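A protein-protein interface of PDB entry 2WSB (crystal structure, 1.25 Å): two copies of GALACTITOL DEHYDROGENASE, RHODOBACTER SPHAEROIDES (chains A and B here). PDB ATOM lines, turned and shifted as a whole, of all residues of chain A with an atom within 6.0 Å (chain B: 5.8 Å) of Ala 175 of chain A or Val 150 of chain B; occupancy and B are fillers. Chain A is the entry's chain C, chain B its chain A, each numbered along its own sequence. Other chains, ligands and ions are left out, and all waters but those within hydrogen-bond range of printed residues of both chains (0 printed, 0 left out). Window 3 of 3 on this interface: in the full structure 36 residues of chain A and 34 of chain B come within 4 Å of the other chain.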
ATOM      1  N   GLN A 168       3.693 -17.137 -23.831  1.00  0.00           N
ATOM      2  CA  GLN A 168       2.953 -15.987 -23.301  1.00  0.00           C
ATOM      3  C   GLN A 168       3.806 -14.720 -23.174  1.00  0.00           C
ATOM      4  O   GLN A 168       3.309 -13.646 -23.399  1.00  0.00           O
ATOM      5  CB  GLN A 168       2.353 -16.278 -21.884  1.00  0.00           C
ATOM      6  CG  GLN A 168       1.072 -17.085 -22.018  1.00  0.00           C
ATOM      7  CD  GLN A 168      -0.047 -16.235 -22.682  1.00  0.00           C
ATOM      8  OE1 GLN A 168      -0.709 -15.356 -22.009  1.00  0.00           O
ATOM      9  NE2 GLN A 168      -0.219 -16.397 -23.963  1.00  0.00           N
ATOM     10  N   THR A 170       6.047 -13.864 -25.407  1.00  0.00           N
ATOM     11  CA  THR A 170       5.974 -13.420 -26.815  1.00  0.00           C
ATOM     12  C   THR A 170       4.699 -12.609 -27.016  1.00  0.00           C
ATOM     13  O   THR A 170       4.705 -11.506 -27.577  1.00  0.00           O
ATOM     14  CB  THR A 170       5.879 -14.637 -27.713  1.00  0.00           C
ATOM     15  OG1 THR A 170       7.133 -15.410 -27.639  1.00  0.00           O
ATOM     16  CG2 THR A 170       5.672 -14.266 -29.181  1.00  0.00           C
ATOM     17  N   ARG A 171       3.562 -13.202 -26.568  1.00  0.00           N
ATOM     18  CA  ARG A 171       2.277 -12.539 -26.761  1.00  0.00           C
ATOM     19  C   ARG A 171       2.131 -11.192 -25.955  1.00  0.00           C
ATOM     20  O   ARG A 171       1.605 -10.239 -26.455  1.00  0.00           O
ATOM     21  CB  ARG A 171       1.179 -13.579 -26.451  1.00  0.00           C
ATOM     22  CG  ARG A 171       1.213 -14.632 -27.559  1.00  0.00           C
ATOM     23  CD  ARG A 171       0.502 -15.912 -27.152  1.00  0.00           C
ATOM     24  NE  ARG A 171      -0.912 -15.735 -26.772  1.00  0.00           N
ATOM     25  CZ  ARG A 171      -1.913 -15.625 -27.697  1.00  0.00           C
ATOM     26  NH1 ARG A 171      -1.625 -15.444 -28.981  1.00  0.00           N
ATOM     27  NH2 ARG A 171      -3.234 -15.605 -27.272  1.00  0.00           N
ATOM     28  N   ALA A 172       2.684 -11.229 -24.735  1.00  0.00           N
ATOM     29  CA  ALA A 172       2.613 -10.013 -23.922  1.00  0.00           C
ATOM     30  C   ALA A 172       3.409  -8.843 -24.558  1.00  0.00           C
ATOM     31  O   ALA A 172       2.902  -7.721 -24.611  1.00  0.00           O
ATOM     32  CB  ALA A 172       3.255 -10.344 -22.535  1.00  0.00           C
ATOM     33  N   LEU A 173       4.604  -9.182 -25.058  1.00  0.00           N
ATOM     34  CA  LEU A 173       5.376  -8.062 -25.691  1.00  0.00           C
ATOM     35  C   LEU A 173       4.723  -7.723 -27.024  1.00  0.00           C
ATOM     36  O   LEU A 173       4.786  -6.534 -27.394  1.00  0.00           O
ATOM     37  CB  LEU A 173       6.857  -8.482 -25.866  1.00  0.00           C
ATOM     38  CG  LEU A 173       7.578  -8.772 -24.555  1.00  0.00           C
ATOM     39  CD1 LEU A 173       9.014  -9.128 -24.817  1.00  0.00           C
ATOM     40  CD2 LEU A 173       7.489  -7.531 -23.591  1.00  0.00           C
ATOM     41  N   ALA A 174       4.165  -8.670 -27.773  1.00  0.00           N
ATOM     42  CA  ALA A 174       3.470  -8.298 -29.032  1.00  0.00           C
ATOM     43  C   ALA A 174       2.360  -7.304 -28.675  1.00  0.00           C
ATOM     44  O   ALA A 174       2.187  -6.290 -29.416  1.00  0.00           O
ATOM     45  CB  ALA A 174       2.847  -9.572 -29.633  1.00  0.00           C
ATOM     46  N   ALA A 175       1.580  -7.537 -27.623  1.00  0.00           N
ATOM     47  CA  ALA A 175       0.478  -6.627 -27.309  1.00  0.00           C
ATOM     48  C   ALA A 175       1.022  -5.287 -26.876  1.00  0.00           C
ATOM     49  O   ALA A 175       0.488  -4.212 -27.246  1.00  0.00           O
ATOM     50  CB  ALA A 175      -0.401  -7.193 -26.177  1.00  0.00           C
ATOM     51  N   GLU A 176       2.061  -5.264 -26.071  1.00  0.00           N
ATOM     52  CA  GLU A 176       2.549  -4.000 -25.476  1.00  0.00           C
ATOM     53  C   GLU A 176       3.241  -3.158 -26.502  1.00  0.00           C
ATOM     54  O   GLU A 176       3.180  -1.908 -26.401  1.00  0.00           O
ATOM     55  CB  GLU A 176       3.504  -4.376 -24.311  1.00  0.00           C
ATOM     56  CG  GLU A 176       3.980  -3.125 -23.568  1.00  0.00           C
ATOM     57  CD  GLU A 176       4.581  -3.401 -22.260  1.00  0.00           C
ATOM     58  OE1 GLU A 176       4.535  -4.522 -21.689  1.00  0.00           O
ATOM     59  OE2 GLU A 176       5.214  -2.403 -21.642  1.00  0.00           O
ATOM     60  N   TRP A 177       3.869  -3.738 -27.536  1.00  0.00           N
ATOM     61  CA  TRP A 177       4.656  -2.975 -28.477  1.00  0.00           C
ATOM     62  C   TRP A 177       3.968  -2.876 -29.862  1.00  0.00           C
ATOM     63  O   TRP A 177       4.522  -2.192 -30.762  1.00  0.00           O
ATOM     64  CB  TRP A 177       6.028  -3.566 -28.648  1.00  0.00           C
ATOM     65  CG  TRP A 177       6.853  -3.462 -27.367  1.00  0.00           C
ATOM     66  CD1 TRP A 177       6.664  -2.569 -26.276  1.00  0.00           C
ATOM     67  CD2 TRP A 177       8.017  -4.254 -27.049  1.00  0.00           C
ATOM     68  NE1 TRP A 177       7.668  -2.813 -25.347  1.00  0.00           N
ATOM     69  CE2 TRP A 177       8.476  -3.838 -25.757  1.00  0.00           C
ATOM     70  CE3 TRP A 177       8.722  -5.244 -27.718  1.00  0.00           C
ATOM     71  CZ2 TRP A 177       9.643  -4.374 -25.140  1.00  0.00           C
ATOM     72  CZ3 TRP A 177       9.832  -5.815 -27.070  1.00  0.00           C
ATOM     73  CH2 TRP A 177      10.323  -5.363 -25.816  1.00  0.00           C
ATOM     74  N   ALA A 178       2.733  -3.425 -30.015  1.00  0.00           N
ATOM     75  CA  ALA A 178       2.078  -3.390 -31.325  1.00  0.00           C
ATOM     76  C   ALA A 178       1.864  -1.938 -31.809  1.00  0.00           C
ATOM     77  O   ALA A 178       2.093  -1.700 -33.000  1.00  0.00           O
ATOM     78  CB  ALA A 178       0.745  -4.109 -31.282  1.00  0.00           C
ATOM     79  N   GLY A 179       1.504  -1.006 -30.939  1.00  0.00           N
ATOM     80  CA  GLY A 179       1.253   0.343 -31.354  1.00  0.00           C
ATOM     81  C   GLY A 179       2.511   1.110 -31.681  1.00  0.00           C
ATOM     82  O   GLY A 179       2.372   2.176 -32.270  1.00  0.00           O
ATOM     83  N   THR A 241       1.479 -10.739 -35.546  1.00  0.00           N
ATOM     84  CA  THR A 241       2.123 -10.441 -34.258  1.00  0.00           C
ATOM     85  C   THR A 241       1.413 -11.222 -33.177  1.00  0.00           C
ATOM     86  O   THR A 241       0.180 -11.392 -33.204  1.00  0.00           O
ATOM     87  CB  THR A 241       2.226  -8.904 -33.999  1.00  0.00           C
ATOM     88  OG1 THR A 241       3.196  -8.765 -32.963  1.00  0.00           O
ATOM     89  CG2 THR A 241       0.888  -8.365 -33.526  1.00  0.00           C
ATOM     90  N   MET B 145      -6.841 -16.478 -17.077  1.00  0.00           N
ATOM     91  CA  MET B 145      -6.946 -16.163 -18.483  1.00  0.00           C
ATOM     92  C   MET B 145      -5.645 -15.547 -19.057  1.00  0.00           C
ATOM     93  O   MET B 145      -5.367 -15.634 -20.259  1.00  0.00           O
ATOM     94  CB  MET B 145      -8.075 -15.181 -18.729  1.00  0.00           C
ATOM     95  CG  MET B 145      -7.911 -13.810 -18.132  1.00  0.00           C
ATOM     96  SD  MET B 145      -9.397 -12.897 -18.590  1.00  0.00           S
ATOM     97  CE  MET B 145      -8.866 -11.162 -18.183  1.00  0.00           C
ATOM     98  N   SER B 146      -4.838 -14.931 -18.171  1.00  0.00           N
ATOM     99  CA  SER B 146      -3.528 -14.370 -18.525  1.00  0.00           C
ATOM    100  C   SER B 146      -2.496 -15.394 -18.879  1.00  0.00           C
ATOM    101  O   SER B 146      -1.390 -15.035 -19.297  1.00  0.00           O
ATOM    102  CB  SER B 146      -2.944 -13.574 -17.339  1.00  0.00           C
ATOM    103  OG  SER B 146      -3.872 -12.566 -16.939  1.00  0.00           O
ATOM    104  N   THR B 148      -3.440 -17.573 -21.274  1.00  0.00           N
ATOM    105  CA  THR B 148      -3.999 -17.844 -22.589  1.00  0.00           C
ATOM    106  C   THR B 148      -3.960 -16.606 -23.456  1.00  0.00           C
ATOM    107  O   THR B 148      -3.608 -16.673 -24.646  1.00  0.00           O
ATOM    108  CB  THR B 148      -5.524 -18.277 -22.429  1.00  0.00           C
ATOM    109  OG1 THR B 148      -5.552 -19.386 -21.481  1.00  0.00           O
ATOM    110  CG2 THR B 148      -6.145 -18.675 -23.750  1.00  0.00           C
ATOM    111  N   ILE B 149      -4.359 -15.439 -22.928  1.00  0.00           N
ATOM    112  CA  ILE B 149      -4.417 -14.139 -23.608  1.00  0.00           C
ATOM    113  C   ILE B 149      -3.617 -13.161 -22.787  1.00  0.00           C
ATOM    114  O   ILE B 149      -2.987 -13.527 -21.748  1.00  0.00           O
ATOM    115  CB  ILE B 149      -5.911 -13.674 -23.832  1.00  0.00           C
ATOM    116  CG1 ILE B 149      -6.768 -13.620 -22.577  1.00  0.00           C
ATOM    117  CG2 ILE B 149      -6.536 -14.623 -24.910  1.00  0.00           C
ATOM    118  CD1 ILE B 149      -6.399 -12.496 -21.566  1.00  0.00           C
ATOM    119  N   VAL B 150      -3.594 -11.906 -23.255  1.00  0.00           N
ATOM    120  CA  VAL B 150      -2.899 -10.826 -22.598  1.00  0.00           C
ATOM    121  C   VAL B 150      -3.908  -9.770 -22.192  1.00  0.00           C
ATOM    122  O   VAL B 150      -4.708  -9.322 -22.998  1.00  0.00           O
ATOM    123  CB  VAL B 150      -1.821 -10.240 -23.560  1.00  0.00           C
ATOM    124  CG1 VAL B 150      -1.111  -9.049 -22.885  1.00  0.00           C
ATOM    125  CG2 VAL B 150      -0.766 -11.300 -23.895  1.00  0.00           C
ATOM    126  N   ASN B 151      -3.803  -9.370 -20.895  1.00  0.00           N
ATOM    127  CA  ASN B 151      -4.720  -8.381 -20.429  1.00  0.00           C
ATOM    128  C   ASN B 151      -4.608  -6.987 -21.072  1.00  0.00           C
ATOM    129  O   ASN B 151      -3.560  -6.694 -21.693  1.00  0.00           O
ATOM    130  CB  ASN B 151      -4.541  -8.161 -18.893  1.00  0.00           C
ATOM    131  CG  ASN B 151      -4.733  -9.399 -18.143  1.00  0.00           C
ATOM    132  OD1 ASN B 151      -5.733  -9.496 -17.339  1.00  0.00           O
ATOM    133  ND2 ASN B 151      -3.898 -10.274 -18.307  1.00  0.00           N
ATOM    134  N   ARG B 152      -5.624  -6.123 -20.981  1.00  0.00           N
ATOM    135  CA  ARG B 152      -5.544  -4.758 -21.457  1.00  0.00           C
ATOM    136  C   ARG B 152      -6.392  -3.916 -20.523  1.00  0.00           C
ATOM    137  O   ARG B 152      -7.443  -4.360 -19.999  1.00  0.00           O
ATOM    138  CB  ARG B 152      -6.001  -4.716 -22.915  1.00  0.00           C
ATOM    139  CG  ARG B 152      -7.392  -5.108 -23.085  1.00  0.00           C
ATOM    140  CD  ARG B 152      -7.839  -5.087 -24.565  1.00  0.00           C
ATOM    141  NE  ARG B 152      -7.870  -3.630 -24.968  1.00  0.00           N
ATOM    142  CZ  ARG B 152      -8.593  -3.128 -25.954  1.00  0.00           C
ATOM    143  NH1 ARG B 152      -9.285  -3.963 -26.728  1.00  0.00           N
ATOM    144  NH2 ARG B 152      -8.497  -1.875 -26.259  1.00  0.00           N
ATOM    145  N   PHE B 155      -0.167  -3.284 -18.434  1.00  0.00           N
ATOM    146  CA  PHE B 155       0.893  -4.185 -18.796  1.00  0.00           C
ATOM    147  C   PHE B 155       1.478  -4.786 -17.565  1.00  0.00           C
ATOM    148  O   PHE B 155       1.697  -4.185 -16.517  1.00  0.00           O
ATOM    149  CB  PHE B 155       1.997  -3.403 -19.560  1.00  0.00           C
ATOM    150  CG  PHE B 155       1.450  -2.766 -20.823  1.00  0.00           C
ATOM    151  CD1 PHE B 155       1.571  -1.410 -21.014  1.00  0.00           C
ATOM    152  CD2 PHE B 155       0.842  -3.584 -21.807  1.00  0.00           C
ATOM    153  CE1 PHE B 155       0.943  -0.772 -22.231  1.00  0.00           C
ATOM    154  CE2 PHE B 155       0.330  -3.037 -22.954  1.00  0.00           C
ATOM    155  CZ  PHE B 155       0.399  -1.769 -23.159  1.00  0.00           C
ATOM    156  N   MET B 160       1.879 -12.451 -17.332  1.00  0.00           N
ATOM    157  CA  MET B 160       1.437 -13.301 -18.472  1.00  0.00           C
ATOM    158  C   MET B 160       2.400 -14.435 -18.645  1.00  0.00           C
ATOM    159  O   MET B 160       1.973 -15.611 -18.796  1.00  0.00           O
ATOM    160  CB  MET B 160       1.455 -12.410 -19.746  1.00  0.00           C
ATOM    161  CG  MET B 160       0.769 -10.986 -19.638  1.00  0.00           C
ATOM    162  SD  MET B 160      -0.923 -11.089 -19.080  1.00  0.00           S
ATOM    163  CE  MET B 160      -0.903  -9.550 -18.041  1.00  0.00           C
ATOM    164  N   TYR B 251     -14.506 -14.145 -21.199  1.00  0.00           N
ATOM    165  CA  TYR B 251     -13.457 -13.187 -21.628  1.00  0.00           C
ATOM    166  C   TYR B 251     -12.652 -13.757 -22.812  1.00  0.00           C
ATOM    167  O   TYR B 251     -12.413 -13.008 -23.786  1.00  0.00           O
ATOM    168  CB  TYR B 251     -12.524 -12.847 -20.459  1.00  0.00           C
ATOM    169  CG  TYR B 251     -11.656 -11.703 -20.732  1.00  0.00           C
ATOM    170  CD1 TYR B 251     -11.971 -10.458 -20.284  1.00  0.00           C
ATOM    171  CD2 TYR B 251     -10.508 -11.802 -21.545  1.00  0.00           C
ATOM    172  CE1 TYR B 251     -11.210  -9.296 -20.563  1.00  0.00           C
ATOM    173  CE2 TYR B 251      -9.660 -10.721 -21.859  1.00  0.00           C
ATOM    174  CZ  TYR B 251     -10.033  -9.458 -21.334  1.00  0.00           C
ATOM    175  OH  TYR B 251      -9.253  -8.343 -21.622  1.00  0.00           O
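SD of Met 160 of chain B sits close to ND2 of Asn 151 of chain B (3.2 Å). OG of Ser 146 of chain B is in hydrogen-bond range of ND2 of Asn 151 of chain B (2.7 Å). The side-chain amide nitrogen of Gln 168 of chain A sits close to the guanidinium group of Arg 171 of chain A.
Thr 170 of chain A touches none of the printed residues of chain B. Printed residues of chain B within 4 Å of Arg 171 of chain A: Thr 148 (2.9 Å) and Val 150 (3.6 Å). Ala 174 of chain A touches none of the printed residues of chain B. Of chain B, only Val 150 (3.8 Å) comes within 4 Å of Ala 175 of chain A. Of the printed residues of chain A, Ser 146 of chain B touches Gln 168 (2.8 Å). Printed residues of chain A within 4 Å of Thr 148 of chain B: Gln 168 and Arg 171. Val 150 of chain B touches just these residues of chain A: Arg 171 (3.6 Å), Ala 172 (3.6 Å) and Ala 175 (3.8 Å).
No position is printed for both chains. Of the 10 pairs that touch across the chains among the printed residues, none has its exchanged pair printed and touching as well.
The side-chain amide oxygen (OE1) of Gln 168 of chain A lies close to the backbone carbonyl oxygen (O) of Ser 146 of chain B (2.8 Å). The guanidinium group of Arg 171 of chain A is in hydrogen-bond range of the backbone carbonyl oxygen of Thr 148 of chain B, 2.9 Å away. O of Ile 149 of chain B lies close to OE1 of Gln 168 of chain A (2.9 Å). O of Thr 148 of chain B lies within hydrogen-bond range of NE2 of Gln 168 of chain A, 3.5 Å away.
Among the printed residues, merely in contact across the chains: Gln 168 of chain A with Met 160 of chain B, Glu 176 of chain A with Phe 155 of chain B, Ala 172 of chain A with Val 150 of chain B, Arg 171 of chain A with Val 150 of chain B, Ala 175 of chain A with Val 150 of chain B and Ala 172 of chain A with Met 160 of chain B.
Of the 10 printed residues of chain B, 6 touch a printed residue of chain A. Printed residues of chain B that touch a printed residue of chain A: Ser 146, Thr 148, Ile 149, Val 150, Phe 155 and Met 160. Hydrophobic or aromatic side chains of chain B within 4 Å of the printed part of chain A: Val 150, Phe 155 and Met 160. Of the 12 printed residues of chain A, 5 touch a printed residue of chain B. Printed residues of chain A that touch a printed residue of chain B: Gln 168, Arg 171, Ala 172, Ala 175 and Glu 176. Among the printed residues, 10 pairs touch across the chains.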
